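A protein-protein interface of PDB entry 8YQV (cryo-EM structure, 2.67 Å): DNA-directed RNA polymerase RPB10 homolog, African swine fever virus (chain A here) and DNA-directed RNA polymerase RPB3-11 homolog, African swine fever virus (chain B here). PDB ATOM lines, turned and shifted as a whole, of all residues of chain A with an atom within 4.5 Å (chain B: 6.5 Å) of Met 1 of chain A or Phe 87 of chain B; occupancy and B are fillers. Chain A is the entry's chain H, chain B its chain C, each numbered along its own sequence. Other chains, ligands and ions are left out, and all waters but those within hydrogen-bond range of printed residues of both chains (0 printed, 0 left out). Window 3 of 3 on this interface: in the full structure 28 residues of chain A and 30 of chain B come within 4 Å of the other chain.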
ATOM      1  N   MET A   1     -24.308 -22.089  24.988  1.00  0.00           N
ATOM      2  CA  MET A   1     -24.404 -22.980  23.846  1.00  0.00           C
ATOM      3  C   MET A   1     -23.475 -22.530  22.736  1.00  0.00           C
ATOM      4  O   MET A   1     -23.322 -23.211  21.732  1.00  0.00           O
ATOM      5  CB  MET A   1     -25.840 -23.045  23.336  1.00  0.00           C
ATOM      6  CG  MET A   1     -26.869 -23.361  24.402  1.00  0.00           C
ATOM      7  SD  MET A   1     -28.465 -23.779  23.697  1.00  0.00           S
ATOM      8  CE  MET A   1     -29.511 -22.576  24.489  1.00  0.00           C
ATOM      9  N   LEU A   2     -22.854 -21.371  22.925  1.00  0.00           N
ATOM     10  CA  LEU A   2     -21.910 -20.812  21.971  1.00  0.00           C
ATOM     11  C   LEU A   2     -20.819 -20.090  22.743  1.00  0.00           C
ATOM     12  O   LEU A   2     -20.882 -19.961  23.964  1.00  0.00           O
ATOM     13  CB  LEU A   2     -22.591 -19.846  20.999  1.00  0.00           C
ATOM     14  CG  LEU A   2     -23.571 -20.394  19.972  1.00  0.00           C
ATOM     15  CD1 LEU A   2     -24.499 -19.303  19.507  1.00  0.00           C
ATOM     16  CD2 LEU A   2     -22.823 -20.984  18.810  1.00  0.00           C
ATOM     17  N   LEU A  74     -17.773 -24.386  25.344  1.00  0.00           N
ATOM     18  CA  LEU A  74     -18.288 -25.509  24.573  1.00  0.00           C
ATOM     19  C   LEU A  74     -19.357 -25.048  23.594  1.00  0.00           C
ATOM     20  O   LEU A  74     -20.279 -24.319  23.965  1.00  0.00           O
ATOM     21  CB  LEU A  74     -18.869 -26.572  25.502  1.00  0.00           C
ATOM     22  CG  LEU A  74     -17.932 -27.258  26.485  1.00  0.00           C
ATOM     23  CD1 LEU A  74     -18.719 -28.194  27.354  1.00  0.00           C
ATOM     24  CD2 LEU A  74     -16.852 -27.997  25.752  1.00  0.00           C
ATOM     25  N   ASP A  75     -19.239 -25.493  22.350  1.00  0.00           N
ATOM     26  CA  ASP A  75     -20.233 -25.199  21.331  1.00  0.00           C
ATOM     27  C   ASP A  75     -21.290 -26.292  21.318  1.00  0.00           C
ATOM     28  O   ASP A  75     -20.964 -27.479  21.254  1.00  0.00           O
ATOM     29  CB  ASP A  75     -19.561 -25.090  19.966  1.00  0.00           C
ATOM     30  CG  ASP A  75     -20.458 -24.490  18.921  1.00  0.00           C
ATOM     31  OD1 ASP A  75     -21.603 -24.135  19.249  1.00  0.00           O
ATOM     32  OD2 ASP A  75     -20.016 -24.370  17.764  1.00  0.00           O
ATOM     33  N   TYR A  76     -22.557 -25.892  21.386  1.00  0.00           N
ATOM     34  CA  TYR A  76     -23.661 -26.840  21.398  1.00  0.00           C
ATOM     35  C   TYR A  76     -23.898 -27.480  20.041  1.00  0.00           C
ATOM     36  O   TYR A  76     -24.479 -28.566  19.980  1.00  0.00           O
ATOM     37  CB  TYR A  76     -24.937 -26.143  21.859  1.00  0.00           C
ATOM     38  CG  TYR A  76     -25.989 -27.044  22.456  1.00  0.00           C
ATOM     39  CD1 TYR A  76     -25.785 -27.662  23.675  1.00  0.00           C
ATOM     40  CD2 TYR A  76     -27.199 -27.256  21.811  1.00  0.00           C
ATOM     41  CE1 TYR A  76     -26.749 -28.474  24.230  1.00  0.00           C
ATOM     42  CE2 TYR A  76     -28.168 -28.068  22.357  1.00  0.00           C
ATOM     43  CZ  TYR A  76     -27.937 -28.674  23.567  1.00  0.00           C
ATOM     44  OH  TYR A  76     -28.897 -29.487  24.118  1.00  0.00           O
ATOM     45  N   TYR A  80     -24.855 -32.031  19.551  1.00  0.00           N
ATOM     46  CA  TYR A  80     -26.267 -32.282  19.311  1.00  0.00           C
ATOM     47  C   TYR A  80     -26.581 -32.240  17.821  1.00  0.00           C
ATOM     48  O   TYR A  80     -26.846 -31.177  17.261  1.00  0.00           O
ATOM     49  CB  TYR A  80     -27.120 -31.260  20.062  1.00  0.00           C
ATOM     50  CG  TYR A  80     -28.606 -31.508  19.977  1.00  0.00           C
ATOM     51  CD1 TYR A  80     -29.205 -32.511  20.722  1.00  0.00           C
ATOM     52  CD2 TYR A  80     -29.411 -30.734  19.157  1.00  0.00           C
ATOM     53  CE1 TYR A  80     -30.561 -32.739  20.650  1.00  0.00           C
ATOM     54  CE2 TYR A  80     -30.769 -30.954  19.078  1.00  0.00           C
ATOM     55  CZ  TYR A  80     -31.340 -31.957  19.827  1.00  0.00           C
ATOM     56  OH  TYR A  80     -32.695 -32.180  19.752  1.00  0.00           O
ATOM     57  N   THR B  84     -40.355 -21.067  15.790  1.00  0.00           N
ATOM     58  CA  THR B  84     -40.590 -22.483  16.010  1.00  0.00           C
ATOM     59  C   THR B  84     -39.403 -23.200  16.638  1.00  0.00           C
ATOM     60  O   THR B  84     -39.560 -24.348  17.066  1.00  0.00           O
ATOM     61  CB  THR B  84     -40.969 -23.163  14.692  1.00  0.00           C
ATOM     62  OG1 THR B  84     -39.951 -22.922  13.719  1.00  0.00           O
ATOM     63  CG2 THR B  84     -42.280 -22.623  14.170  1.00  0.00           C
ATOM     64  N   ASP B  85     -38.232 -22.573  16.714  1.00  0.00           N
ATOM     65  CA  ASP B  85     -37.073 -23.250  17.276  1.00  0.00           C
ATOM     66  C   ASP B  85     -37.206 -23.389  18.782  1.00  0.00           C
ATOM     67  O   ASP B  85     -37.681 -22.482  19.469  1.00  0.00           O
ATOM     68  CB  ASP B  85     -35.778 -22.515  16.947  1.00  0.00           C
ATOM     69  CG  ASP B  85     -34.560 -23.397  17.136  1.00  0.00           C
ATOM     70  OD1 ASP B  85     -34.266 -24.205  16.236  1.00  0.00           O
ATOM     71  OD2 ASP B  85     -33.910 -23.305  18.195  1.00  0.00           O
ATOM     72  N   LEU B  86     -36.760 -24.530  19.293  1.00  0.00           N
ATOM     73  CA  LEU B  86     -36.974 -24.882  20.687  1.00  0.00           C
ATOM     74  C   LEU B  86     -35.805 -24.518  21.586  1.00  0.00           C
ATOM     75  O   LEU B  86     -36.019 -24.197  22.759  1.00  0.00           O
ATOM     76  CB  LEU B  86     -37.256 -26.380  20.800  1.00  0.00           C
ATOM     77  CG  LEU B  86     -38.586 -26.846  20.211  1.00  0.00           C
ATOM     78  CD1 LEU B  86     -38.680 -28.348  20.265  1.00  0.00           C
ATOM     79  CD2 LEU B  86     -39.756 -26.207  20.945  1.00  0.00           C
ATOM     80  N   PHE B  87     -34.576 -24.560  21.071  1.00  0.00           N
ATOM     81  CA  PHE B  87     -33.406 -24.285  21.894  1.00  0.00           C
ATOM     82  C   PHE B  87     -33.095 -22.805  22.016  1.00  0.00           C
ATOM     83  O   PHE B  87     -32.544 -22.381  23.036  1.00  0.00           O
ATOM     84  CB  PHE B  87     -32.184 -25.018  21.341  1.00  0.00           C
ATOM     85  CG  PHE B  87     -32.313 -26.505  21.376  1.00  0.00           C
ATOM     86  CD1 PHE B  87     -32.035 -27.204  22.531  1.00  0.00           C
ATOM     87  CD2 PHE B  87     -32.731 -27.202  20.261  1.00  0.00           C
ATOM     88  CE1 PHE B  87     -32.164 -28.571  22.572  1.00  0.00           C
ATOM     89  CE2 PHE B  87     -32.864 -28.566  20.296  1.00  0.00           C
ATOM     90  CZ  PHE B  87     -32.579 -29.252  21.452  1.00  0.00           C
ATOM     91  N   MET B  88     -33.436 -22.003  21.009  1.00  0.00           N
ATOM     92  CA  MET B  88     -33.143 -20.573  21.040  1.00  0.00           C
ATOM     93  C   MET B  88     -34.261 -19.867  21.795  1.00  0.00           C
ATOM     94  O   MET B  88     -35.114 -19.186  21.225  1.00  0.00           O
ATOM     95  CB  MET B  88     -32.981 -20.024  19.630  1.00  0.00           C
ATOM     96  CG  MET B  88     -31.807 -20.612  18.875  1.00  0.00           C
ATOM     97  SD  MET B  88     -30.199 -20.123  19.520  1.00  0.00           S
ATOM     98  CE  MET B  88     -29.688 -21.608  20.363  1.00  0.00           C
ATOM     99  N   THR B  89     -34.243 -20.028  23.113  1.00  0.00           N
ATOM    100  CA  THR B  89     -35.262 -19.413  23.943  1.00  0.00           C
ATOM    101  C   THR B  89     -35.100 -17.897  23.933  1.00  0.00           C
ATOM    102  O   THR B  89     -34.091 -17.356  23.487  1.00  0.00           O
ATOM    103  CB  THR B  89     -35.193 -19.955  25.367  1.00  0.00           C
ATOM    104  OG1 THR B  89     -33.941 -19.602  25.956  1.00  0.00           O
ATOM    105  CG2 THR B  89     -35.308 -21.456  25.359  1.00  0.00           C
ATOM    106  N   GLU B  90     -36.129 -17.203  24.413  1.00  0.00           N
ATOM    107  CA  GLU B  90     -36.081 -15.746  24.415  1.00  0.00           C
ATOM    108  C   GLU B  90     -35.006 -15.231  25.356  1.00  0.00           C
ATOM    109  O   GLU B  90     -34.364 -14.220  25.070  1.00  0.00           O
ATOM    110  CB  GLU B  90     -37.439 -15.165  24.798  1.00  0.00           C
ATOM    111  CG  GLU B  90     -37.456 -13.649  24.831  1.00  0.00           C
ATOM    112  CD  GLU B  90     -38.819 -13.082  25.156  1.00  0.00           C
ATOM    113  OE1 GLU B  90     -39.763 -13.874  25.343  1.00  0.00           O
ATOM    114  OE2 GLU B  90     -38.948 -11.843  25.227  1.00  0.00           O
ATOM    115  N   PHE B  92     -32.101 -16.680  26.169  1.00  0.00           N
ATOM    116  CA  PHE B  92     -30.796 -16.862  25.547  1.00  0.00           C
ATOM    117  C   PHE B  92     -30.532 -15.791  24.498  1.00  0.00           C
ATOM    118  O   PHE B  92     -29.494 -15.124  24.524  1.00  0.00           O
ATOM    119  CB  PHE B  92     -30.716 -18.258  24.932  1.00  0.00           C
ATOM    120  CG  PHE B  92     -29.377 -18.596  24.353  1.00  0.00           C
ATOM    121  CD1 PHE B  92     -28.316 -18.923  25.173  1.00  0.00           C
ATOM    122  CD2 PHE B  92     -29.181 -18.598  22.988  1.00  0.00           C
ATOM    123  CE1 PHE B  92     -27.092 -19.240  24.642  1.00  0.00           C
ATOM    124  CE2 PHE B  92     -27.952 -18.912  22.456  1.00  0.00           C
ATOM    125  CZ  PHE B  92     -26.911 -19.234  23.284  1.00  0.00           C
ATOM    126  N   ILE B  93     -31.472 -15.598  23.574  1.00  0.00           N
ATOM    127  CA  ILE B  93     -31.263 -14.646  22.489  1.00  0.00           C
ATOM    128  C   ILE B  93     -31.253 -13.214  23.002  1.00  0.00           C
ATOM    129  O   ILE B  93     -30.511 -12.373  22.488  1.00  0.00           O
ATOM    130  CB  ILE B  93     -32.320 -14.846  21.394  1.00  0.00           C
ATOM    131  CG1 ILE B  93     -32.305 -16.285  20.904  1.00  0.00           C
ATOM    132  CG2 ILE B  93     -32.039 -13.941  20.233  1.00  0.00           C
ATOM    133  CD1 ILE B  93     -31.055 -16.650  20.174  1.00  0.00           C
ATOM    134  N   ARG B  96     -27.908 -12.655  24.374  1.00  0.00           N
ATOM    135  CA  ARG B  96     -26.972 -12.534  23.261  1.00  0.00           C
ATOM    136  C   ARG B  96     -27.019 -11.144  22.641  1.00  0.00           C
ATOM    137  O   ARG B  96     -25.977 -10.567  22.323  1.00  0.00           O
ATOM    138  CB  ARG B  96     -27.282 -13.584  22.195  1.00  0.00           C
ATOM    139  CG  ARG B  96     -27.021 -15.007  22.610  1.00  0.00           C
ATOM    140  CD  ARG B  96     -25.589 -15.155  22.954  1.00  0.00           C
ATOM    141  NE  ARG B  96     -24.739 -15.144  21.775  1.00  0.00           N
ATOM    142  CZ  ARG B  96     -23.747 -15.993  21.573  1.00  0.00           C
ATOM    143  NH1 ARG B  96     -23.415 -16.887  22.484  1.00  0.00           N
ATOM    144  NH2 ARG B  96     -23.045 -15.912  20.451  1.00  0.00           N
ATOM    145  N   PHE B 151     -28.405 -20.323  16.439  1.00  0.00           N
ATOM    146  CA  PHE B 151     -28.432 -21.353  15.411  1.00  0.00           C
ATOM    147  C   PHE B 151     -29.785 -22.047  15.428  1.00  0.00           C
ATOM    148  O   PHE B 151     -30.412 -22.181  16.481  1.00  0.00           O
ATOM    149  CB  PHE B 151     -27.298 -22.371  15.583  1.00  0.00           C
ATOM    150  CG  PHE B 151     -27.272 -23.052  16.918  1.00  0.00           C
ATOM    151  CD1 PHE B 151     -26.580 -22.501  17.976  1.00  0.00           C
ATOM    152  CD2 PHE B 151     -27.904 -24.263  17.105  1.00  0.00           C
ATOM    153  CE1 PHE B 151     -26.544 -23.129  19.199  1.00  0.00           C
ATOM    154  CE2 PHE B 151     -27.865 -24.894  18.325  1.00  0.00           C
ATOM    155  CZ  PHE B 151     -27.185 -24.326  19.371  1.00  0.00           C
ATOM    156  N   GLN B 153     -32.183 -25.396  14.162  1.00  0.00           N
ATOM    157  CA  GLN B 153     -32.296 -26.765  13.697  1.00  0.00           C
ATOM    158  C   GLN B 153     -33.005 -26.788  12.346  1.00  0.00           C
ATOM    159  O   GLN B 153     -33.690 -25.829  11.985  1.00  0.00           O
ATOM    160  CB  GLN B 153     -33.064 -27.606  14.711  1.00  0.00           C
ATOM    161  CG  GLN B 153     -32.530 -27.543  16.124  1.00  0.00           C
ATOM    162  CD  GLN B 153     -31.101 -28.016  16.236  1.00  0.00           C
ATOM    163  OE1 GLN B 153     -30.687 -28.946  15.552  1.00  0.00           O
ATOM    164  NE2 GLN B 153     -30.336 -27.378  17.108  1.00  0.00           N
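Among the printed residues, merely in contact across the chains: Met 1 of chain A with Phe 87 of chain B, Met 1 of chain A with Phe 92 of chain B, Leu 2 of chain A with Arg 96 of chain B, Tyr 76 of chain A with Phe 87 of chain B, Tyr 76 of chain A with Phe 151 of chain B and Tyr 80 of chain A with Phe 87 of chain B.
The side-chain hydroxyl of Thr 89 of chain B lies within hydrogen-bond range of the backbone NH of Phe 92 of chain B.
The side-chain carboxylate (OD2) of Asp 85 of chain B sits at hydrogen-bond distance from the backbone NH (N) of Phe 87 of chain B (3.2 Å).
O of Met 1 of chain A is in hydrogen-bond range of N of Tyr 76 of chain A, 2.8 Å away.
The backbone NH (N) of Phe 151 of chain B is in hydrogen-bond range of the side-chain sulfur (SD) of Met 88 of chain B.
Printed residues of chain B that touch a printed residue of chain A: Phe 87, Phe 92, Arg 96 and Phe 151.
Hydrophobic or aromatic side chains of chain B that line the printed part of chain A: Phe 87, Phe 92 and Phe 151.
Of the 6 printed residues of chain A, 4 touch a printed residue of chain B.
Printed residues of chain A that touch a printed residue of chain B: Met 1, Leu 2, Tyr 76 and Tyr 80.
Hydrophobic or aromatic side chains of chain A that line the printed part of chain B: Met 1, Leu 2, Tyr 76 and Tyr 80.
Along chain A the printed residues that touch a printed residue of chain B span positions 1 to 80.
Among the printed residues, 6 pairs touch across the chains.
Met 1 of chain A touches two residues of chain B.
Phe 87 of chain B touches just these residues of chain A: Met 1, Tyr 76 and Tyr 80.
Of the printed residues of chain A, Arg 96 of chain B touches Leu 2.
Printed residues of chain A within 4 Å of Phe 151 of chain B: Tyr 76.
Of the printed residues of chain B, Tyr 80 of chain A touches Phe 87.
Of the printed residues of chain A, Phe 92 of chain B touches Met 1.
Printed residues of chain B within 4 Å of Tyr 76 of chain A: Phe 87 and Phe 151.
The nearest residue of chain B that does not touch Met 1 of chain A is Phe 151 of chain B (4.1 Å).
The nearest printed residue of chain B that does not touch Tyr 80 of chain A is Gln 153 of chain B (4.04 Å).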
